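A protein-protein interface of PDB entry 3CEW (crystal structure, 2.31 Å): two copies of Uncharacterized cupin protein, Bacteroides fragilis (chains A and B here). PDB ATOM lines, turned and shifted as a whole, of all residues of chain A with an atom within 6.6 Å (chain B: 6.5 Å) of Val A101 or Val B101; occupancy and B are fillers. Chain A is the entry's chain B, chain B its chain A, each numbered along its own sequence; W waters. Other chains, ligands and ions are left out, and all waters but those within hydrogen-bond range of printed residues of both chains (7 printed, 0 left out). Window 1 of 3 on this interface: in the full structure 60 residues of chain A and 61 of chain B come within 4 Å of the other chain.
OG1 of Thr B24 sits at hydrogen-bond distance from OE1 of Glu A49 (2.8 Å).
The side-chain hydroxyl (OG1) of Thr B24 is in hydrogen-bond range of the backbone NH (N) of Gly A104 (2.9 Å).
The backbone carbonyl oxygen of Thr B24 is in hydrogen-bond range of the backbone NH of Ser A105 (3.4 Å).
The backbone carbonyl oxygen of Thr B24 is in hydrogen-bond range of the backbone NH of Leu A106 (3.1 Å).
The backbone NH (N) of Gly B25 is in hydrogen-bond range of the side-chain carboxylate (OE2) of Glu A49.
The side-chain carboxylate (OE1) of Glu B49 lies within hydrogen-bond range of the side-chain hydroxyl (OG1) of Thr A24, 2.8 Å away.
The backbone NH (N) of Gly A25 lies within hydrogen-bond range of the side-chain carboxylate (OE2) of Glu B49.
The backbone NH of Gly B104 lies within hydrogen-bond range of the side-chain hydroxyl of Thr A24 (3.0 Å).
The backbone carbonyl oxygen (O) of Thr A24 lies within hydrogen-bond range of the backbone NH (N) of Ser B105, 3.4 Å away.
The backbone NH (N) of Leu B106 is in hydrogen-bond range of the backbone carbonyl oxygen (O) of Thr A24 (3.1 Å).
The backbone NH of Glu B49 sits at hydrogen-bond distance from the backbone carbonyl oxygen of Val B101 (2.6 Å).
The backbone carbonyl oxygen (O) of Lys B102 sits at hydrogen-bond distance from the side-chain hydroxyl (OG) of Ser B105 (2.7 Å).
O of Gln A47 is in hydrogen-bond range of N of Ala A103, at 2.9 Å.
N of Glu A49 is in hydrogen-bond range of O of Val A101 (2.6 Å).
O of Ile A51 is in hydrogen-bond range of N of Ile A99 (2.8 Å).
O of Lys A102 lies within hydrogen-bond range of OG of Ser A105, at 2.7 Å.
Gly A25 touches Val B101 (CA to CG2, 3.5 Å).
CA of Gly A25 touches O of Lys B102, at 3.7 Å.
C of Gly A25 touches CB of Leu B106, 3.8 Å away.
Leu B106 touches Ala A26.
CD1 of Ile A99 touches CD1 of Ile B99, at 3.2 Å.
Val B101 touches Val A101 (CG1 to CG1, 3.6 Å).
CA of Ala A103 touches OG1 of Thr B24 (3.7 Å).
Ser A105 touches Ser B105 (OG to OG, 3.6 Å).
Gly B25 touches Leu A106 (C to CB, 3.7 Å).
CD2 of Leu A106 touches O of Ala B26, at 3.4 Å.
Printed residues of chain A within 4 Å of Ser B105: Thr A24, Lys A102 and Ser A105.
Of the printed residues of chain B, Ala A103 touches Thr B24.
Asn A48 touches none of the printed residues of chain B.
Glu A27 touches none of the printed residues of chain B.
The nearest printed residue of chain B that does not touch Ala A103 is Gly B25 (4.8 Å).
Of the 17 printed residues of chain B, 12 touch a printed residue of chain A.
Of the 17 printed residues of chain A, 11 touch a printed residue of chain B.
Hydrophobic or aromatic side chains of chain A that line the printed part of chain B: Ile A99, Val A101, Ala A103 and Leu A106.
Among the printed residues, no Asp or Glu carboxylate lies within 4 Å of a Lys or Arg side-chain nitrogen of the other chain.
Thr A24 touches Glu B49, and with the chains exchanged Glu A49 touches Thr B24.
Thr A24 touches Gly B104, and with the chains exchanged Gly A104 touches Thr B24.
Gly A25 touches Lys B102, and with the chains exchanged Lys A102 touches Gly B25.
Ile B99 touches its own counterpart, Ile A99.
Positions printed for both chains: 24, 25, 26, 27, 47, 48, 49, 50, 51, 99, 100, 101, 102, 103, 104, 105 and 106.
Of the 26 pairs that touch across the chains among the printed residues, 25 have their exchanged pair printed and touching as well.
Water W2 lies within hydrogen-bond range of the backbone carbonyl oxygen (O) of Thr B24 (2.7 Å) and the backbone carbonyl oxygen (O) of Leu A106 (2.7 Å).
Water W1 lies within hydrogen-bond range of OG of Ser A105 (2.7 Å), N of Lys B102 (2.9 Å), O of Gly B25 (3.0 Å) and OG of Ser B105 (3.4 Å).
Water W6 lies within hydrogen-bond range of the backbone carbonyl oxygen of Gly A25, the side-chain hydroxyl of Ser B105, the backbone NH of Lys A102 and the backbone NH of Leu B106.
Water W5 bridges O of Ser B105 (2.8 Å) and NZ of Lys A102 (3.2 Å).
Water W4 lies within hydrogen-bond range of O of Ser A105 and NZ of Lys B102.
Water W3 bridges the side-chain hydroxyl of Thr A24 (3.4 Å) and the backbone NH of Gly B104 (3.4 Å).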
ATOM      1  N   THR A  24     -20.426 -11.410  -5.598  1.00  0.00           N
ATOM      2  CA  THR A  24     -19.779 -12.715  -5.714  1.00  0.00           C
ATOM      3  C   THR A  24     -19.989 -13.541  -4.449  1.00  0.00           C
ATOM      4  O   THR A  24     -19.686 -14.731  -4.415  1.00  0.00           O
ATOM      5  CB  THR A  24     -18.258 -12.584  -5.951  1.00  0.00           C
ATOM      6  OG1 THR A  24     -17.642 -12.017  -4.785  1.00  0.00           O
ATOM      7  CG2 THR A  24     -17.977 -11.715  -7.178  1.00  0.00           C
ATOM      8  N   GLY A  25     -20.519 -12.907  -3.409  1.00  0.00           N
ATOM      9  CA  GLY A  25     -20.730 -13.616  -2.159  1.00  0.00           C
ATOM     10  C   GLY A  25     -22.176 -13.753  -1.747  1.00  0.00           C
ATOM     11  O   GLY A  25     -22.484 -14.388  -0.738  1.00  0.00           O
ATOM     12  N   ALA A  26     -23.073 -13.166  -2.523  1.00  0.00           N
ATOM     13  CA  ALA A  26     -24.481 -13.242  -2.187  1.00  0.00           C
ATOM     14  C   ALA A  26     -25.378 -12.724  -3.292  1.00  0.00           C
ATOM     15  O   ALA A  26     -24.917 -12.232  -4.321  1.00  0.00           O
ATOM     16  CB  ALA A  26     -24.744 -12.436  -0.923  1.00  0.00           C
ATOM     17  N   GLU A  27     -26.674 -12.873  -3.068  1.00  0.00           N
ATOM     18  CA  GLU A  27     -27.684 -12.341  -3.963  1.00  0.00           C
ATOM     19  C   GLU A  27     -28.568 -11.602  -2.981  1.00  0.00           C
ATOM     20  O   GLU A  27     -28.837 -12.108  -1.885  1.00  0.00           O
ATOM     21  CB  GLU A  27     -28.483 -13.441  -4.666  1.00  0.00           C
ATOM     22  CG  GLU A  27     -29.821 -12.969  -5.285  1.00  0.00           C
ATOM     23  CD  GLU A  27     -29.684 -11.807  -6.281  1.00  0.00           C
ATOM     24  OE1 GLU A  27     -29.282 -10.693  -5.885  1.00  0.00           O
ATOM     25  OE2 GLU A  27     -29.986 -11.999  -7.474  1.00  0.00           O
ATOM     26  N   GLN A  47     -28.472 -25.339  -0.852  1.00  0.00           N
ATOM     27  CA  GLN A  47     -27.300 -25.048  -0.037  1.00  0.00           C
ATOM     28  C   GLN A  47     -27.186 -23.606   0.457  1.00  0.00           C
ATOM     29  O   GLN A  47     -26.244 -23.268   1.176  1.00  0.00           O
ATOM     30  CB  GLN A  47     -26.033 -25.419  -0.808  1.00  0.00           C
ATOM     31  CG  GLN A  47     -25.668 -24.448  -1.912  1.00  0.00           C
ATOM     32  CD  GLN A  47     -24.289 -24.733  -2.495  1.00  0.00           C
ATOM     33  OE1 GLN A  47     -23.664 -23.860  -3.104  1.00  0.00           O
ATOM     34  NE2 GLN A  47     -23.814 -25.968  -2.318  1.00  0.00           N
ATOM     35  N   ASN A  48     -28.133 -22.756   0.083  1.00  0.00           N
ATOM     36  CA  ASN A  48     -28.089 -21.366   0.516  1.00  0.00           C
ATOM     37  C   ASN A  48     -28.908 -21.038   1.753  1.00  0.00           C
ATOM     38  O   ASN A  48     -30.083 -21.387   1.858  1.00  0.00           O
ATOM     39  CB  ASN A  48     -28.540 -20.424  -0.606  1.00  0.00           C
ATOM     40  CG  ASN A  48     -27.515 -20.298  -1.703  1.00  0.00           C
ATOM     41  OD1 ASN A  48     -26.339 -20.625  -1.516  1.00  0.00           O
ATOM     42  ND2 ASN A  48     -27.947 -19.802  -2.856  1.00  0.00           N
ATOM     43  N   GLU A  49     -28.259 -20.354   2.684  1.00  0.00           N
ATOM     44  CA  GLU A  49     -28.897 -19.884   3.899  1.00  0.00           C
ATOM     45  C   GLU A  49     -29.597 -18.610   3.431  1.00  0.00           C
ATOM     46  O   GLU A  49     -29.138 -17.958   2.504  1.00  0.00           O
ATOM     47  CB  GLU A  49     -27.825 -19.564   4.945  1.00  0.00           C
ATOM     48  CG  GLU A  49     -28.262 -18.685   6.093  1.00  0.00           C
ATOM     49  CD  GLU A  49     -27.147 -18.486   7.105  1.00  0.00           C
ATOM     50  OE1 GLU A  49     -26.918 -19.401   7.924  1.00  0.00           O
ATOM     51  OE2 GLU A  49     -26.478 -17.430   7.065  1.00  0.00           O
ATOM     52  N   GLU A  50     -30.713 -18.264   4.047  1.00  0.00           N
ATOM     53  CA  GLU A  50     -31.421 -17.066   3.647  1.00  0.00           C
ATOM     54  C   GLU A  50     -31.691 -16.180   4.857  1.00  0.00           C
ATOM     55  O   GLU A  50     -32.088 -16.664   5.927  1.00  0.00           O
ATOM     56  CB  GLU A  50     -32.717 -17.456   2.930  1.00  0.00           C
ATOM     57  CG  GLU A  50     -33.107 -16.520   1.808  1.00  0.00           C
ATOM     58  CD  GLU A  50     -33.951 -17.189   0.718  1.00  0.00           C
ATOM     59  OE1 GLU A  50     -35.009 -17.770   1.026  1.00  0.00           O
ATOM     60  OE2 GLU A  50     -33.558 -17.114  -0.462  1.00  0.00           O
ATOM     61  N   ILE A  51     -31.437 -14.885   4.694  1.00  0.00           N
ATOM     62  CA  ILE A  51     -31.640 -13.917   5.766  1.00  0.00           C
ATOM     63  C   ILE A  51     -32.706 -12.924   5.317  1.00  0.00           C
ATOM     64  O   ILE A  51     -32.572 -12.271   4.280  1.00  0.00           O
ATOM     65  CB  ILE A  51     -30.335 -13.161   6.064  1.00  0.00           C
ATOM     66  CG1 ILE A  51     -29.219 -14.166   6.376  1.00  0.00           C
ATOM     67  CG2 ILE A  51     -30.514 -12.224   7.252  1.00  0.00           C
ATOM     68  CD1 ILE A  51     -27.835 -13.594   6.257  1.00  0.00           C
ATOM     69  N   ILE A  99     -31.538 -11.907   1.691  1.00  0.00           N
ATOM     70  CA  ILE A  99     -30.118 -12.080   1.449  1.00  0.00           C
ATOM     71  C   ILE A  99     -29.839 -13.572   1.345  1.00  0.00           C
ATOM     72  O   ILE A  99     -30.066 -14.341   2.286  1.00  0.00           O
ATOM     73  CB  ILE A  99     -29.278 -11.497   2.589  1.00  0.00           C
ATOM     74  CG1 ILE A  99     -29.616 -10.018   2.788  1.00  0.00           C
ATOM     75  CG2 ILE A  99     -27.807 -11.650   2.271  1.00  0.00           C
ATOM     76  CD1 ILE A  99     -29.017  -9.439   4.051  1.00  0.00           C
ATOM     77  N   GLN A 100     -29.351 -13.971   0.179  1.00  0.00           N
ATOM     78  CA  GLN A 100     -29.046 -15.360  -0.093  1.00  0.00           C
ATOM     79  C   GLN A 100     -27.525 -15.564  -0.068  1.00  0.00           C
ATOM     80  O   GLN A 100     -26.787 -14.893  -0.797  1.00  0.00           O
ATOM     81  CB  GLN A 100     -29.632 -15.705  -1.459  1.00  0.00           C
ATOM     82  CG  GLN A 100     -29.977 -17.147  -1.681  1.00  0.00           C
ATOM     83  CD  GLN A 100     -30.600 -17.380  -3.046  1.00  0.00           C
ATOM     84  OE1 GLN A 100     -30.458 -18.457  -3.618  1.00  0.00           O
ATOM     85  NE2 GLN A 100     -31.304 -16.371  -3.570  1.00  0.00           N
ATOM     86  N   VAL A 101     -27.062 -16.471   0.792  1.00  0.00           N
ATOM     87  CA  VAL A 101     -25.640 -16.768   0.913  1.00  0.00           C
ATOM     88  C   VAL A 101     -25.437 -18.271   1.117  1.00  0.00           C
ATOM     89  O   VAL A 101     -26.298 -18.954   1.676  1.00  0.00           O
ATOM     90  CB  VAL A 101     -24.988 -16.015   2.112  1.00  0.00           C
ATOM     91  CG1 VAL A 101     -25.104 -14.510   1.912  1.00  0.00           C
ATOM     92  CG2 VAL A 101     -25.648 -16.429   3.433  1.00  0.00           C
ATOM     93  N   LYS A 102     -24.300 -18.785   0.661  1.00  0.00           N
ATOM     94  CA  LYS A 102     -24.020 -20.203   0.817  1.00  0.00           C
ATOM     95  C   LYS A 102     -23.835 -20.524   2.295  1.00  0.00           C
ATOM     96  O   LYS A 102     -22.954 -19.977   2.951  1.00  0.00           O
ATOM     97  CB  LYS A 102     -22.765 -20.601   0.028  1.00  0.00           C
ATOM     98  CG  LYS A 102     -22.507 -22.102   0.033  1.00  0.00           C
ATOM     99  CD  LYS A 102     -21.240 -22.479  -0.723  1.00  0.00           C
ATOM    100  CE  LYS A 102     -20.957 -23.972  -0.582  1.00  0.00           C
ATOM    101  NZ  LYS A 102     -19.647 -24.320  -1.197  1.00  0.00           N
ATOM    102  N   ALA A 103     -24.674 -21.418   2.806  1.00  0.00           N
ATOM    103  CA  ALA A 103     -24.617 -21.825   4.205  1.00  0.00           C
ATOM    104  C   ALA A 103     -23.249 -22.387   4.584  1.00  0.00           C
ATOM    105  O   ALA A 103     -22.667 -23.164   3.832  1.00  0.00           O
ATOM    106  CB  ALA A 103     -25.707 -22.862   4.487  1.00  0.00           C
ATOM    107  N   GLY A 104     -22.746 -21.977   5.749  1.00  0.00           N
ATOM    108  CA  GLY A 104     -21.459 -22.447   6.234  1.00  0.00           C
ATOM    109  C   GLY A 104     -20.242 -21.924   5.491  1.00  0.00           C
ATOM    110  O   GLY A 104     -19.126 -22.356   5.766  1.00  0.00           O
ATOM    111  N   SER A 105     -20.437 -20.990   4.565  1.00  0.00           N
ATOM    112  CA  SER A 105     -19.317 -20.462   3.790  1.00  0.00           C
ATOM    113  C   SER A 105     -18.522 -19.363   4.504  1.00  0.00           C
ATOM    114  O   SER A 105     -17.358 -19.117   4.183  1.00  0.00           O
ATOM    115  CB  SER A 105     -19.818 -19.920   2.452  1.00  0.00           C
ATOM    116  OG  SER A 105     -20.600 -18.748   2.631  1.00  0.00           O
ATOM    117  N   LEU A 106     -19.147 -18.698   5.467  1.00  0.00           N
ATOM    118  CA  LEU A 106     -18.462 -17.637   6.187  1.00  0.00           C
ATOM    119  C   LEU A 106     -17.352 -18.155   7.103  1.00  0.00           C
ATOM    120  O   LEU A 106     -17.539 -19.122   7.846  1.00  0.00           O
ATOM    121  CB  LEU A 106     -19.463 -16.838   7.016  1.00  0.00           C
ATOM    122  CG  LEU A 106     -18.865 -15.600   7.689  1.00  0.00           C
ATOM    123  CD1 LEU A 106     -18.457 -14.587   6.616  1.00  0.00           C
ATOM    124  CD2 LEU A 106     -19.889 -14.981   8.638  1.00  0.00           C
ATOM    125  N   THR B  24     -24.442 -18.463   9.345  1.00  0.00           N
ATOM    126  CA  THR B  24     -23.295 -19.277   8.957  1.00  0.00           C
ATOM    127  C   THR B  24     -22.761 -18.838   7.602  1.00  0.00           C
ATOM    128  O   THR B  24     -21.694 -19.270   7.182  1.00  0.00           O
ATOM    129  CB  THR B  24     -23.657 -20.787   8.869  1.00  0.00           C
ATOM    130  OG1 THR B  24     -24.584 -20.995   7.795  1.00  0.00           O
ATOM    131  CG2 THR B  24     -24.270 -21.275  10.175  1.00  0.00           C
ATOM    132  N   GLY B  25     -23.505 -17.978   6.919  1.00  0.00           N
ATOM    133  CA  GLY B  25     -23.061 -17.529   5.612  1.00  0.00           C
ATOM    134  C   GLY B  25     -22.760 -16.046   5.522  1.00  0.00           C
ATOM    135  O   GLY B  25     -22.338 -15.560   4.477  1.00  0.00           O
ATOM    136  N   ALA B  26     -22.971 -15.319   6.610  1.00  0.00           N
ATOM    137  CA  ALA B  26     -22.717 -13.889   6.597  1.00  0.00           C
ATOM    138  C   ALA B  26     -22.802 -13.271   7.967  1.00  0.00           C
ATOM    139  O   ALA B  26     -23.143 -13.931   8.947  1.00  0.00           O
ATOM    140  CB  ALA B  26     -23.724 -13.199   5.678  1.00  0.00           C
ATOM    141  N   GLU B  27     -22.465 -11.991   8.018  1.00  0.00           N
ATOM    142  CA  GLU B  27     -22.581 -11.206   9.231  1.00  0.00           C
ATOM    143  C   GLU B  27     -23.343  -9.999   8.720  1.00  0.00           C
ATOM    144  O   GLU B  27     -23.056  -9.492   7.632  1.00  0.00           O
ATOM    145  CB  GLU B  27     -21.217 -10.772   9.782  1.00  0.00           C
ATOM    146  CG  GLU B  27     -21.274  -9.601  10.794  1.00  0.00           C
ATOM    147  CD  GLU B  27     -22.192  -9.850  12.003  1.00  0.00           C
ATOM    148  OE1 GLU B  27     -23.422  -9.994  11.836  1.00  0.00           O
ATOM    149  OE2 GLU B  27     -21.679  -9.895  13.138  1.00  0.00           O
ATOM    150  N   GLN B  47     -10.729 -11.238   3.025  1.00  0.00           N
ATOM    151  CA  GLN B  47     -11.413 -12.090   2.065  1.00  0.00           C
ATOM    152  C   GLN B  47     -12.926 -11.886   1.966  1.00  0.00           C
ATOM    153  O   GLN B  47     -13.595 -12.552   1.174  1.00  0.00           O
ATOM    154  CB  GLN B  47     -11.120 -13.554   2.379  1.00  0.00           C
ATOM    155  CG  GLN B  47     -11.858 -14.092   3.592  1.00  0.00           C
ATOM    156  CD  GLN B  47     -11.719 -15.603   3.737  1.00  0.00           C
ATOM    157  OE1 GLN B  47     -12.529 -16.257   4.404  1.00  0.00           O
ATOM    158  NE2 GLN B  47     -10.682 -16.163   3.120  1.00  0.00           N
ATOM    159  N   ASN B  48     -13.470 -10.968   2.756  1.00  0.00           N
ATOM    160  CA  ASN B  48     -14.903 -10.729   2.707  1.00  0.00           C
ATOM    161  C   ASN B  48     -15.350  -9.571   1.828  1.00  0.00           C
ATOM    162  O   ASN B  48     -14.826  -8.458   1.915  1.00  0.00           O
ATOM    163  CB  ASN B  48     -15.468 -10.490   4.109  1.00  0.00           C
ATOM    164  CG  ASN B  48     -15.534 -11.754   4.939  1.00  0.00           C
ATOM    165  OD1 ASN B  48     -15.500 -12.864   4.407  1.00  0.00           O
ATOM    166  ND2 ASN B  48     -15.652 -11.590   6.253  1.00  0.00           N
ATOM    167  N   GLU B  49     -16.323  -9.863   0.979  1.00  0.00           N
ATOM    168  CA  GLU B  49     -16.936  -8.863   0.127  1.00  0.00           C
ATOM    169  C   GLU B  49     -17.908  -8.152   1.071  1.00  0.00           C
ATOM    170  O   GLU B  49     -18.408  -8.750   2.018  1.00  0.00           O
ATOM    171  CB  GLU B  49     -17.690  -9.561  -1.003  1.00  0.00           C
ATOM    172  CG  GLU B  49     -18.724  -8.726  -1.728  1.00  0.00           C
ATOM    173  CD  GLU B  49     -19.341  -9.492  -2.899  1.00  0.00           C
ATOM    174  OE1 GLU B  49     -18.695  -9.600  -3.960  1.00  0.00           O
ATOM    175  OE2 GLU B  49     -20.463 -10.011  -2.753  1.00  0.00           O
ATOM    176  N   GLU B  50     -18.170  -6.874   0.836  1.00  0.00           N
ATOM    177  CA  GLU B  50     -19.091  -6.158   1.700  1.00  0.00           C
ATOM    178  C   GLU B  50     -20.166  -5.466   0.870  1.00  0.00           C
ATOM    179  O   GLU B  50     -19.882  -4.864  -0.166  1.00  0.00           O
ATOM    180  CB  GLU B  50     -18.307  -5.165   2.566  1.00  0.00           C
ATOM    181  CG  GLU B  50     -18.873  -4.994   3.953  1.00  0.00           C
ATOM    182  CD  GLU B  50     -17.835  -4.563   4.994  1.00  0.00           C
ATOM    183  OE1 GLU B  50     -17.164  -3.532   4.806  1.00  0.00           O
ATOM    184  OE2 GLU B  50     -17.700  -5.262   6.014  1.00  0.00           O
ATOM    185  N   ILE B  51     -21.411  -5.585   1.319  1.00  0.00           N
ATOM    186  CA  ILE B  51     -22.541  -4.990   0.626  1.00  0.00           C
ATOM    187  C   ILE B  51     -23.181  -3.976   1.562  1.00  0.00           C
ATOM    188  O   ILE B  51     -23.578  -4.304   2.683  1.00  0.00           O
ATOM    189  CB  ILE B  51     -23.574  -6.071   0.249  1.00  0.00           C
ATOM    190  CG1 ILE B  51     -22.889  -7.170  -0.564  1.00  0.00           C
ATOM    191  CG2 ILE B  51     -24.699  -5.466  -0.576  1.00  0.00           C
ATOM    192  CD1 ILE B  51     -23.674  -8.466  -0.616  1.00  0.00           C
ATOM    193  N   ILE B  99     -23.555  -5.941   4.952  1.00  0.00           N
ATOM    194  CA  ILE B  99     -23.603  -7.382   4.805  1.00  0.00           C
ATOM    195  C   ILE B  99     -22.202  -7.854   4.439  1.00  0.00           C
ATOM    196  O   ILE B  99     -21.641  -7.464   3.412  1.00  0.00           O
ATOM    197  CB  ILE B  99     -24.576  -7.799   3.699  1.00  0.00           C
ATOM    198  CG1 ILE B  99     -25.961  -7.231   3.986  1.00  0.00           C
ATOM    199  CG2 ILE B  99     -24.644  -9.322   3.619  1.00  0.00           C
ATOM    200  CD1 ILE B  99     -26.924  -7.397   2.821  1.00  0.00           C
ATOM    201  N   GLN B 100     -21.647  -8.696   5.297  1.00  0.00           N
ATOM    202  CA  GLN B 100     -20.314  -9.232   5.113  1.00  0.00           C
ATOM    203  C   GLN B 100     -20.416 -10.700   4.685  1.00  0.00           C
ATOM    204  O   GLN B 100     -21.024 -11.513   5.377  1.00  0.00           O
ATOM    205  CB  GLN B 100     -19.564  -9.092   6.441  1.00  0.00           C
ATOM    206  CG  GLN B 100     -18.077  -8.979   6.338  1.00  0.00           C
ATOM    207  CD  GLN B 100     -17.421  -8.770   7.689  1.00  0.00           C
ATOM    208  OE1 GLN B 100     -16.280  -9.177   7.897  1.00  0.00           O
ATOM    209  NE2 GLN B 100     -18.137  -8.141   8.618  1.00  0.00           N
ATOM    210  N   VAL B 101     -19.832 -11.022   3.531  1.00  0.00           N
ATOM    211  CA  VAL B 101     -19.842 -12.383   3.003  1.00  0.00           C
ATOM    212  C   VAL B 101     -18.500 -12.716   2.351  1.00  0.00           C
ATOM    213  O   VAL B 101     -17.819 -11.831   1.819  1.00  0.00           O
ATOM    214  CB  VAL B 101     -20.967 -12.585   1.946  1.00  0.00           C
ATOM    215  CG1 VAL B 101     -22.326 -12.345   2.576  1.00  0.00           C
ATOM    216  CG2 VAL B 101     -20.762 -11.642   0.752  1.00  0.00           C
ATOM    217  N   LYS B 102     -18.117 -13.989   2.398  1.00  0.00           N
ATOM    218  CA  LYS B 102     -16.851 -14.398   1.802  1.00  0.00           C
ATOM    219  C   LYS B 102     -16.917 -14.221   0.289  1.00  0.00           C
ATOM    220  O   LYS B 102     -17.761 -14.821  -0.376  1.00  0.00           O
ATOM    221  CB  LYS B 102     -16.534 -15.857   2.139  1.00  0.00           C
ATOM    222  CG  LYS B 102     -15.144 -16.280   1.673  1.00  0.00           C
ATOM    223  CD  LYS B 102     -14.842 -17.734   1.989  1.00  0.00           C
ATOM    224  CE  LYS B 102     -13.496 -18.141   1.402  1.00  0.00           C
ATOM    225  NZ  LYS B 102     -13.270 -19.604   1.563  1.00  0.00           N
ATOM    226  N   ALA B 103     -16.020 -13.389  -0.236  1.00  0.00           N
ATOM    227  CA  ALA B 103     -15.967 -13.103  -1.657  1.00  0.00           C
ATOM    228  C   ALA B 103     -15.773 -14.368  -2.480  1.00  0.00           C
ATOM    229  O   ALA B 103     -14.952 -15.215  -2.132  1.00  0.00           O
ATOM    230  CB  ALA B 103     -14.838 -12.104  -1.943  1.00  0.00           C
ATOM    231  N   GLY B 104     -16.545 -14.490  -3.561  1.00  0.00           N
ATOM    232  CA  GLY B 104     -16.447 -15.642  -4.451  1.00  0.00           C
ATOM    233  C   GLY B 104     -16.995 -16.945  -3.898  1.00  0.00           C
ATOM    234  O   GLY B 104     -16.845 -17.991  -4.530  1.00  0.00           O
ATOM    235  N   SER B 105     -17.640 -16.895  -2.736  1.00  0.00           N
ATOM    236  CA  SER B 105     -18.176 -18.104  -2.127  1.00  0.00           C
ATOM    237  C   SER B 105     -19.530 -18.532  -2.684  1.00  0.00           C
ATOM    238  O   SER B 105     -19.905 -19.699  -2.586  1.00  0.00           O
ATOM    239  CB  SER B 105     -18.296 -17.924  -0.608  1.00  0.00           C
ATOM    240  OG  SER B 105     -19.313 -16.984  -0.272  1.00  0.00           O
ATOM    241  N   LEU B 106     -20.268 -17.596  -3.262  1.00  0.00           N
ATOM    242  CA  LEU B 106     -21.575 -17.926  -3.801  1.00  0.00           C
ATOM    243  C   LEU B 106     -21.491 -18.801  -5.052  1.00  0.00           C
ATOM    244  O   LEU B 106     -20.701 -18.542  -5.955  1.00  0.00           O
ATOM    245  CB  LEU B 106     -22.339 -16.648  -4.132  1.00  0.00           C
ATOM    246  CG  LEU B 106     -23.790 -16.884  -4.564  1.00  0.00           C
ATOM    247  CD1 LEU B 106     -24.575 -17.429  -3.379  1.00  0.00           C
ATOM    248  CD2 LEU B 106     -24.425 -15.580  -5.051  1.00  0.00           C
HETATM  249  O   HOH W   1     -19.806 -16.211   3.049  1.00  0.00           O
HETATM  250  O   HOH W   2     -19.793 -20.313   8.751  1.00  0.00           O
HETATM  251  O   HOH W   3     -14.503 -12.797  -5.736  1.00  0.00           O
HETATM  252  O   HOH W   4     -15.614 -20.882   2.861  1.00  0.00           O
HETATM  253  O   HOH W   5     -18.085 -21.800  -2.394  1.00  0.00           O
HETATM  254  O   HOH W   6     -22.094 -17.129  -0.421  1.00  0.00           O
HETATM  255  O   HOH W   7     -19.622 -16.008  -6.624  1.00  0.00           O
